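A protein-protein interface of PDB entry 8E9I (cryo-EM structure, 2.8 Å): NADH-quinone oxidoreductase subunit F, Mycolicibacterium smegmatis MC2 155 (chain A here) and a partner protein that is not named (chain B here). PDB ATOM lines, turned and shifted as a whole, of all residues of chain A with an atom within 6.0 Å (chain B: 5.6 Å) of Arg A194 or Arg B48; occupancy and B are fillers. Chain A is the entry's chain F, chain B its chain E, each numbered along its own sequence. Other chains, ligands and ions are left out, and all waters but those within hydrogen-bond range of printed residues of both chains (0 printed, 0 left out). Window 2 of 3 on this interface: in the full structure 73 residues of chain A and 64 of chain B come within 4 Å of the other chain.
O of Gly A193 sits at hydrogen-bond distance from NE of Arg B48 (2.6 Å). The side-chain hydroxyl (OG) of Ser B49 is in hydrogen-bond range of the backbone carbonyl oxygen (O) of Leu A191 (2.5 Å). The backbone carbonyl oxygen (O) of Arg A194 lies within hydrogen-bond range of the side-chain hydroxyl (OH) of Tyr B91 (2.9 Å). OH of Tyr B91 is in hydrogen-bond range of N of Gly A196 (3.1 Å). The backbone carbonyl oxygen (O) of Arg B48 lies close to the backbone carbonyl oxygen (O) of Glu A192. The guanidinium group (NH1) of Arg A194 sits close to the guanidinium group (NH1) of Arg B48 (3.0 Å).
N of Arg A194 is in hydrogen-bond range of O of Asp A189. The side-chain carboxylate of Glu A192 is in salt-bridge range of the guanidinium group of Arg A194 (3.2 Å). OE1 of Glu A192 is in salt-bridge range of NH2 of Arg A199 (3.6 Å).
Among the printed residues, pairs that only touch across the chains: Ser A190 with Tyr B91 (3.0 Å), Gly A193 with Leu B51 (3.2 Å), Ser A190 with Leu B52 (3.5 Å), Glu A192 with Ser B49 (3.6 Å), Gly A193 with Val B87 (3.6 Å), Arg A194 with Val B87 (3.6 Å), Arg A195 with Val B87 (3.7 Å) and Arg A195 with Tyr B91 (3.8 Å).
Of the printed residues of chain B, Arg A194 touches Arg B48 (3.0 Å), Val B87 (3.6 Å) and Tyr B91 (2.9 Å). Arg B48 touches just these residues of chain A: Glu A192 (3.4 Å), Gly A193 (2.6 Å) and Arg A194 (3.0 Å). Of the printed residues of chain B, Leu A191 touches Ser B49. Printed residues of chain A within 4 Å of Leu B52: Ser A190. Printed residues of chain A within 4 Å of Leu B51: Gly A193. Of the printed residues of chain A, Val B87 touches Gly A193 (3.6 Å), Arg A194 (3.6 Å) and Arg A195 (3.7 Å). Printed residues of chain A within 4 Å of Tyr B91: Ser A190 (3.0 Å), Arg A194 (2.9 Å), Arg A195 (3.8 Å) and Gly A196 (3.1 Å). Glu B83 touches none of the printed residues of chain A. Asp B46 touches none of the printed residues of chain A. The nearest residue of chain B that does not touch Arg A194 is Leu B52 (4.6 Å). The nearest residue of chain A that does not touch Arg B48 is Leu A191 (5.2 Å).
Of the 10 printed residues of chain A, 7 touch a printed residue of chain B. Hydrophobic or aromatic side chains of chain A within 4 Å of the printed part of chain B: Leu A191. Of the 12 printed residues of chain B, 6 touch a printed residue of chain A. Among the printed residues, 14 pairs touch across the chains.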
ATOM      1  N   ASP A 189     -28.072   6.923  24.606  1.00  0.00           N
ATOM      2  CA  ASP A 189     -26.766   6.949  25.260  1.00  0.00           C
ATOM      3  C   ASP A 189     -26.876   7.450  26.691  1.00  0.00           C
ATOM      4  O   ASP A 189     -26.223   6.915  27.592  1.00  0.00           O
ATOM      5  CB  ASP A 189     -25.782   7.811  24.476  1.00  0.00           C
ATOM      6  CG  ASP A 189     -25.396   7.193  23.161  1.00  0.00           C
ATOM      7  OD1 ASP A 189     -25.400   5.949  23.068  1.00  0.00           O
ATOM      8  OD2 ASP A 189     -25.073   7.946  22.222  1.00  0.00           O
ATOM      9  N   SER A 190     -27.678   8.487  26.922  1.00  0.00           N
ATOM     10  CA  SER A 190     -27.842   8.962  28.286  1.00  0.00           C
ATOM     11  C   SER A 190     -28.519   7.914  29.153  1.00  0.00           C
ATOM     12  O   SER A 190     -28.224   7.817  30.347  1.00  0.00           O
ATOM     13  CB  SER A 190     -28.640  10.260  28.302  1.00  0.00           C
ATOM     14  OG  SER A 190     -29.973  10.035  27.887  1.00  0.00           O
ATOM     15  N   LEU A 191     -29.427   7.127  28.577  1.00  0.00           N
ATOM     16  CA  LEU A 191     -30.072   6.077  29.354  1.00  0.00           C
ATOM     17  C   LEU A 191     -29.124   4.909  29.572  1.00  0.00           C
ATOM     18  O   LEU A 191     -29.246   4.177  30.561  1.00  0.00           O
ATOM     19  CB  LEU A 191     -31.351   5.615  28.656  1.00  0.00           C
ATOM     20  CG  LEU A 191     -32.231   4.646  29.450  1.00  0.00           C
ATOM     21  CD1 LEU A 191     -33.666   4.799  28.993  1.00  0.00           C
ATOM     22  CD2 LEU A 191     -31.821   3.187  29.308  1.00  0.00           C
ATOM     23  N   GLU A 192     -28.180   4.714  28.658  1.00  0.00           N
ATOM     24  CA  GLU A 192     -27.179   3.672  28.818  1.00  0.00           C
ATOM     25  C   GLU A 192     -26.088   4.054  29.797  1.00  0.00           C
ATOM     26  O   GLU A 192     -25.175   3.254  30.013  1.00  0.00           O
ATOM     27  CB  GLU A 192     -26.554   3.337  27.466  1.00  0.00           C
ATOM     28  CG  GLU A 192     -27.442   2.507  26.568  1.00  0.00           C
ATOM     29  CD  GLU A 192     -26.738   2.073  25.305  1.00  0.00           C
ATOM     30  OE1 GLU A 192     -25.494   1.989  25.315  1.00  0.00           O
ATOM     31  OE2 GLU A 192     -27.428   1.817  24.297  1.00  0.00           O
ATOM     32  N   GLY A 193     -26.156   5.235  30.402  1.00  0.00           N
ATOM     33  CA  GLY A 193     -25.094   5.678  31.279  1.00  0.00           C
ATOM     34  C   GLY A 193     -23.876   6.186  30.544  1.00  0.00           C
ATOM     35  O   GLY A 193     -22.746   5.889  30.945  1.00  0.00           O
ATOM     36  N   ARG A 194     -24.072   6.922  29.459  1.00  0.00           N
ATOM     37  CA  ARG A 194     -22.991   7.543  28.710  1.00  0.00           C
ATOM     38  C   ARG A 194     -23.294   9.020  28.512  1.00  0.00           C
ATOM     39  O   ARG A 194     -24.360   9.515  28.880  1.00  0.00           O
ATOM     40  CB  ARG A 194     -22.784   6.862  27.356  1.00  0.00           C
ATOM     41  CG  ARG A 194     -22.701   5.359  27.428  1.00  0.00           C
ATOM     42  CD  ARG A 194     -22.400   4.777  26.071  1.00  0.00           C
ATOM     43  NE  ARG A 194     -22.712   3.357  26.026  1.00  0.00           N
ATOM     44  CZ  ARG A 194     -21.896   2.400  26.439  1.00  0.00           C
ATOM     45  NH1 ARG A 194     -20.697   2.674  26.926  1.00  0.00           N
ATOM     46  NH2 ARG A 194     -22.295   1.135  26.367  1.00  0.00           N
ATOM     47  N   ARG A 195     -22.330   9.728  27.935  1.00  0.00           N
ATOM     48  CA  ARG A 195     -22.576  11.106  27.557  1.00  0.00           C
ATOM     49  C   ARG A 195     -23.770  11.153  26.621  1.00  0.00           C
ATOM     50  O   ARG A 195     -23.855  10.386  25.659  1.00  0.00           O
ATOM     51  CB  ARG A 195     -21.348  11.707  26.879  1.00  0.00           C
ATOM     52  CG  ARG A 195     -20.126  11.777  27.763  1.00  0.00           C
ATOM     53  CD  ARG A 195     -18.889  12.105  26.956  1.00  0.00           C
ATOM     54  NE  ARG A 195     -18.927  13.452  26.407  1.00  0.00           N
ATOM     55  CZ  ARG A 195     -18.772  14.553  27.127  1.00  0.00           C
ATOM     56  NH1 ARG A 195     -18.603  14.507  28.437  1.00  0.00           N
ATOM     57  NH2 ARG A 195     -18.785  15.733  26.517  1.00  0.00           N
ATOM     58  N   GLY A 196     -24.699  12.054  26.906  1.00  0.00           N
ATOM     59  CA  GLY A 196     -25.907  12.136  26.120  1.00  0.00           C
ATOM     60  C   GLY A 196     -25.664  12.710  24.745  1.00  0.00           C
ATOM     61  O   GLY A 196     -26.266  13.723  24.382  1.00  0.00           O
ATOM     62  N   GLN A 197     -24.785  12.077  23.969  1.00  0.00           N
ATOM     63  CA  GLN A 197     -24.519  12.571  22.628  1.00  0.00           C
ATOM     64  C   GLN A 197     -25.190  11.690  21.588  1.00  0.00           C
ATOM     65  O   GLN A 197     -25.306  10.480  21.784  1.00  0.00           O
ATOM     66  CB  GLN A 197     -23.020  12.611  22.347  1.00  0.00           C
ATOM     67  CG  GLN A 197     -22.249  13.552  23.230  1.00  0.00           C
ATOM     68  CD  GLN A 197     -20.890  13.876  22.661  1.00  0.00           C
ATOM     69  OE1 GLN A 197     -20.305  13.079  21.935  1.00  0.00           O
ATOM     70  NE2 GLN A 197     -20.380  15.053  22.983  1.00  0.00           N
ATOM     71  N   ARG A 199     -25.835   9.334  18.371  1.00  0.00           N
ATOM     72  CA  ARG A 199     -25.048   8.329  17.682  1.00  0.00           C
ATOM     73  C   ARG A 199     -25.094   8.549  16.177  1.00  0.00           C
ATOM     74  O   ARG A 199     -25.765   9.450  15.669  1.00  0.00           O
ATOM     75  CB  ARG A 199     -25.559   6.928  17.995  1.00  0.00           C
ATOM     76  CG  ARG A 199     -25.577   6.554  19.451  1.00  0.00           C
ATOM     77  CD  ARG A 199     -26.325   5.256  19.616  1.00  0.00           C
ATOM     78  NE  ARG A 199     -26.567   4.925  21.013  1.00  0.00           N
ATOM     79  CZ  ARG A 199     -27.143   3.806  21.422  1.00  0.00           C
ATOM     80  NH1 ARG A 199     -27.554   2.888  20.565  1.00  0.00           N
ATOM     81  NH2 ARG A 199     -27.311   3.602  22.723  1.00  0.00           N
ATOM     82  N   ASP B  46     -28.778  -3.323  32.010  1.00  0.00           N
ATOM     83  CA  ASP B  46     -27.325  -3.221  31.969  1.00  0.00           C
ATOM     84  C   ASP B  46     -26.880  -2.404  33.167  1.00  0.00           C
ATOM     85  O   ASP B  46     -27.521  -1.407  33.510  1.00  0.00           O
ATOM     86  CB  ASP B  46     -26.851  -2.575  30.664  1.00  0.00           C
ATOM     87  N   ALA B  47     -25.786  -2.821  33.802  1.00  0.00           N
ATOM     88  CA  ALA B  47     -25.327  -2.123  34.997  1.00  0.00           C
ATOM     89  C   ALA B  47     -25.058  -0.653  34.710  1.00  0.00           C
ATOM     90  O   ALA B  47     -25.560   0.225  35.419  1.00  0.00           O
ATOM     91  CB  ALA B  47     -24.071  -2.798  35.542  1.00  0.00           C
ATOM     92  N   ARG B  48     -24.290  -0.362  33.656  1.00  0.00           N
ATOM     93  CA  ARG B  48     -23.915   1.021  33.387  1.00  0.00           C
ATOM     94  C   ARG B  48     -25.134   1.906  33.202  1.00  0.00           C
ATOM     95  O   ARG B  48     -25.058   3.116  33.424  1.00  0.00           O
ATOM     96  CB  ARG B  48     -23.027   1.117  32.149  1.00  0.00           C
ATOM     97  CG  ARG B  48     -22.450   2.510  31.948  1.00  0.00           C
ATOM     98  CD  ARG B  48     -21.632   2.620  30.685  1.00  0.00           C
ATOM     99  NE  ARG B  48     -21.099   3.966  30.521  1.00  0.00           N
ATOM    100  CZ  ARG B  48     -19.944   4.257  29.939  1.00  0.00           C
ATOM    101  NH1 ARG B  48     -19.170   3.314  29.427  1.00  0.00           N
ATOM    102  NH2 ARG B  48     -19.553   5.525  29.873  1.00  0.00           N
ATOM    103  N   SER B  49     -26.259   1.330  32.793  1.00  0.00           N
ATOM    104  CA  SER B  49     -27.454   2.134  32.597  1.00  0.00           C
ATOM    105  C   SER B  49     -27.812   2.917  33.848  1.00  0.00           C
ATOM    106  O   SER B  49     -28.383   4.005  33.747  1.00  0.00           O
ATOM    107  CB  SER B  49     -28.614   1.232  32.188  1.00  0.00           C
ATOM    108  OG  SER B  49     -29.661   1.976  31.599  1.00  0.00           O
ATOM    109  N   ALA B  50     -27.473   2.392  35.023  1.00  0.00           N
ATOM    110  CA  ALA B  50     -27.795   3.055  36.276  1.00  0.00           C
ATOM    111  C   ALA B  50     -26.779   4.115  36.669  1.00  0.00           C
ATOM    112  O   ALA B  50     -26.742   4.506  37.840  1.00  0.00           O
ATOM    113  CB  ALA B  50     -27.901   2.016  37.386  1.00  0.00           C
ATOM    114  N   LEU B  51     -25.950   4.579  35.736  1.00  0.00           N
ATOM    115  CA  LEU B  51     -24.940   5.573  36.078  1.00  0.00           C
ATOM    116  C   LEU B  51     -25.574   6.902  36.459  1.00  0.00           C
ATOM    117  O   LEU B  51     -25.250   7.474  37.506  1.00  0.00           O
ATOM    118  CB  LEU B  51     -23.977   5.752  34.909  1.00  0.00           C
ATOM    119  CG  LEU B  51     -22.882   6.800  35.087  1.00  0.00           C
ATOM    120  CD1 LEU B  51     -22.119   6.589  36.377  1.00  0.00           C
ATOM    121  CD2 LEU B  51     -21.935   6.756  33.909  1.00  0.00           C
ATOM    122  N   LEU B  52     -26.485   7.410  35.626  1.00  0.00           N
ATOM    123  CA  LEU B  52     -27.101   8.705  35.912  1.00  0.00           C
ATOM    124  C   LEU B  52     -27.811   8.705  37.256  1.00  0.00           C
ATOM    125  O   LEU B  52     -27.590   9.633  38.054  1.00  0.00           O
ATOM    126  CB  LEU B  52     -28.048   9.082  34.772  1.00  0.00           C
ATOM    127  CG  LEU B  52     -27.496  10.077  33.751  1.00  0.00           C
ATOM    128  CD1 LEU B  52     -26.262   9.519  33.080  1.00  0.00           C
ATOM    129  CD2 LEU B  52     -28.552  10.411  32.718  1.00  0.00           C
ATOM    130  N   LEU B  77     -19.806   0.299  38.925  1.00  0.00           N
ATOM    131  CA  LEU B  77     -20.113  -0.017  37.537  1.00  0.00           C
ATOM    132  C   LEU B  77     -18.928  -0.576  36.765  1.00  0.00           C
ATOM    133  O   LEU B  77     -19.041  -0.781  35.554  1.00  0.00           O
ATOM    134  CB  LEU B  77     -20.645   1.232  36.838  1.00  0.00           C
ATOM    135  CG  LEU B  77     -22.138   1.481  37.033  1.00  0.00           C
ATOM    136  CD1 LEU B  77     -22.457   1.708  38.481  1.00  0.00           C
ATOM    137  CD2 LEU B  77     -22.561   2.688  36.229  1.00  0.00           C
ATOM    138  N   LEU B  79     -16.451   0.923  35.766  1.00  0.00           N
ATOM    139  CA  LEU B  79     -15.931   1.921  34.850  1.00  0.00           C
ATOM    140  C   LEU B  79     -14.639   2.523  35.385  1.00  0.00           C
ATOM    141  O   LEU B  79     -14.247   2.308  36.532  1.00  0.00           O
ATOM    142  CB  LEU B  79     -16.947   3.037  34.637  1.00  0.00           C
ATOM    143  CG  LEU B  79     -18.284   2.632  34.037  1.00  0.00           C
ATOM    144  CD1 LEU B  79     -19.264   3.775  34.179  1.00  0.00           C
ATOM    145  CD2 LEU B  79     -18.105   2.251  32.583  1.00  0.00           C
ATOM    146  N   GLU B  83     -14.194   7.798  32.567  1.00  0.00           N
ATOM    147  CA  GLU B  83     -15.486   7.657  31.903  1.00  0.00           C
ATOM    148  C   GLU B  83     -16.608   8.210  32.768  1.00  0.00           C
ATOM    149  O   GLU B  83     -17.526   8.880  32.271  1.00  0.00           O
ATOM    150  CB  GLU B  83     -15.746   6.191  31.567  1.00  0.00           C
ATOM    151  N   VAL B  87     -19.153  11.336  31.796  1.00  0.00           N
ATOM    152  CA  VAL B  87     -20.609  11.346  31.875  1.00  0.00           C
ATOM    153  C   VAL B  87     -21.080  12.446  32.816  1.00  0.00           C
ATOM    154  O   VAL B  87     -21.995  13.212  32.497  1.00  0.00           O
ATOM    155  CB  VAL B  87     -21.135   9.971  32.311  1.00  0.00           C
ATOM    156  CG1 VAL B  87     -22.622  10.040  32.570  1.00  0.00           C
ATOM    157  CG2 VAL B  87     -20.836   8.938  31.252  1.00  0.00           C
ATOM    158  N   TYR B  91     -23.705  16.555  32.093  1.00  0.00           N
ATOM    159  CA  TYR B  91     -25.012  17.036  32.512  1.00  0.00           C
ATOM    160  C   TYR B  91     -24.892  18.166  33.525  1.00  0.00           C
ATOM    161  O   TYR B  91     -24.020  18.166  34.397  1.00  0.00           O
ATOM    162  CB  TYR B  91     -25.833  15.893  33.092  1.00  0.00           C
ATOM    163  CG  TYR B  91     -25.937  14.729  32.151  1.00  0.00           C
ATOM    164  CD1 TYR B  91     -24.963  13.748  32.119  1.00  0.00           C
ATOM    165  CD2 TYR B  91     -27.001  14.621  31.278  1.00  0.00           C
ATOM    166  CE1 TYR B  91     -25.056  12.688  31.249  1.00  0.00           C
ATOM    167  CE2 TYR B  91     -27.097  13.570  30.413  1.00  0.00           C
ATOM    168  CZ  TYR B  91     -26.127  12.609  30.397  1.00  0.00           C
ATOM    169  OH  TYR B  91     -26.242  11.561  29.520  1.00  0.00           O
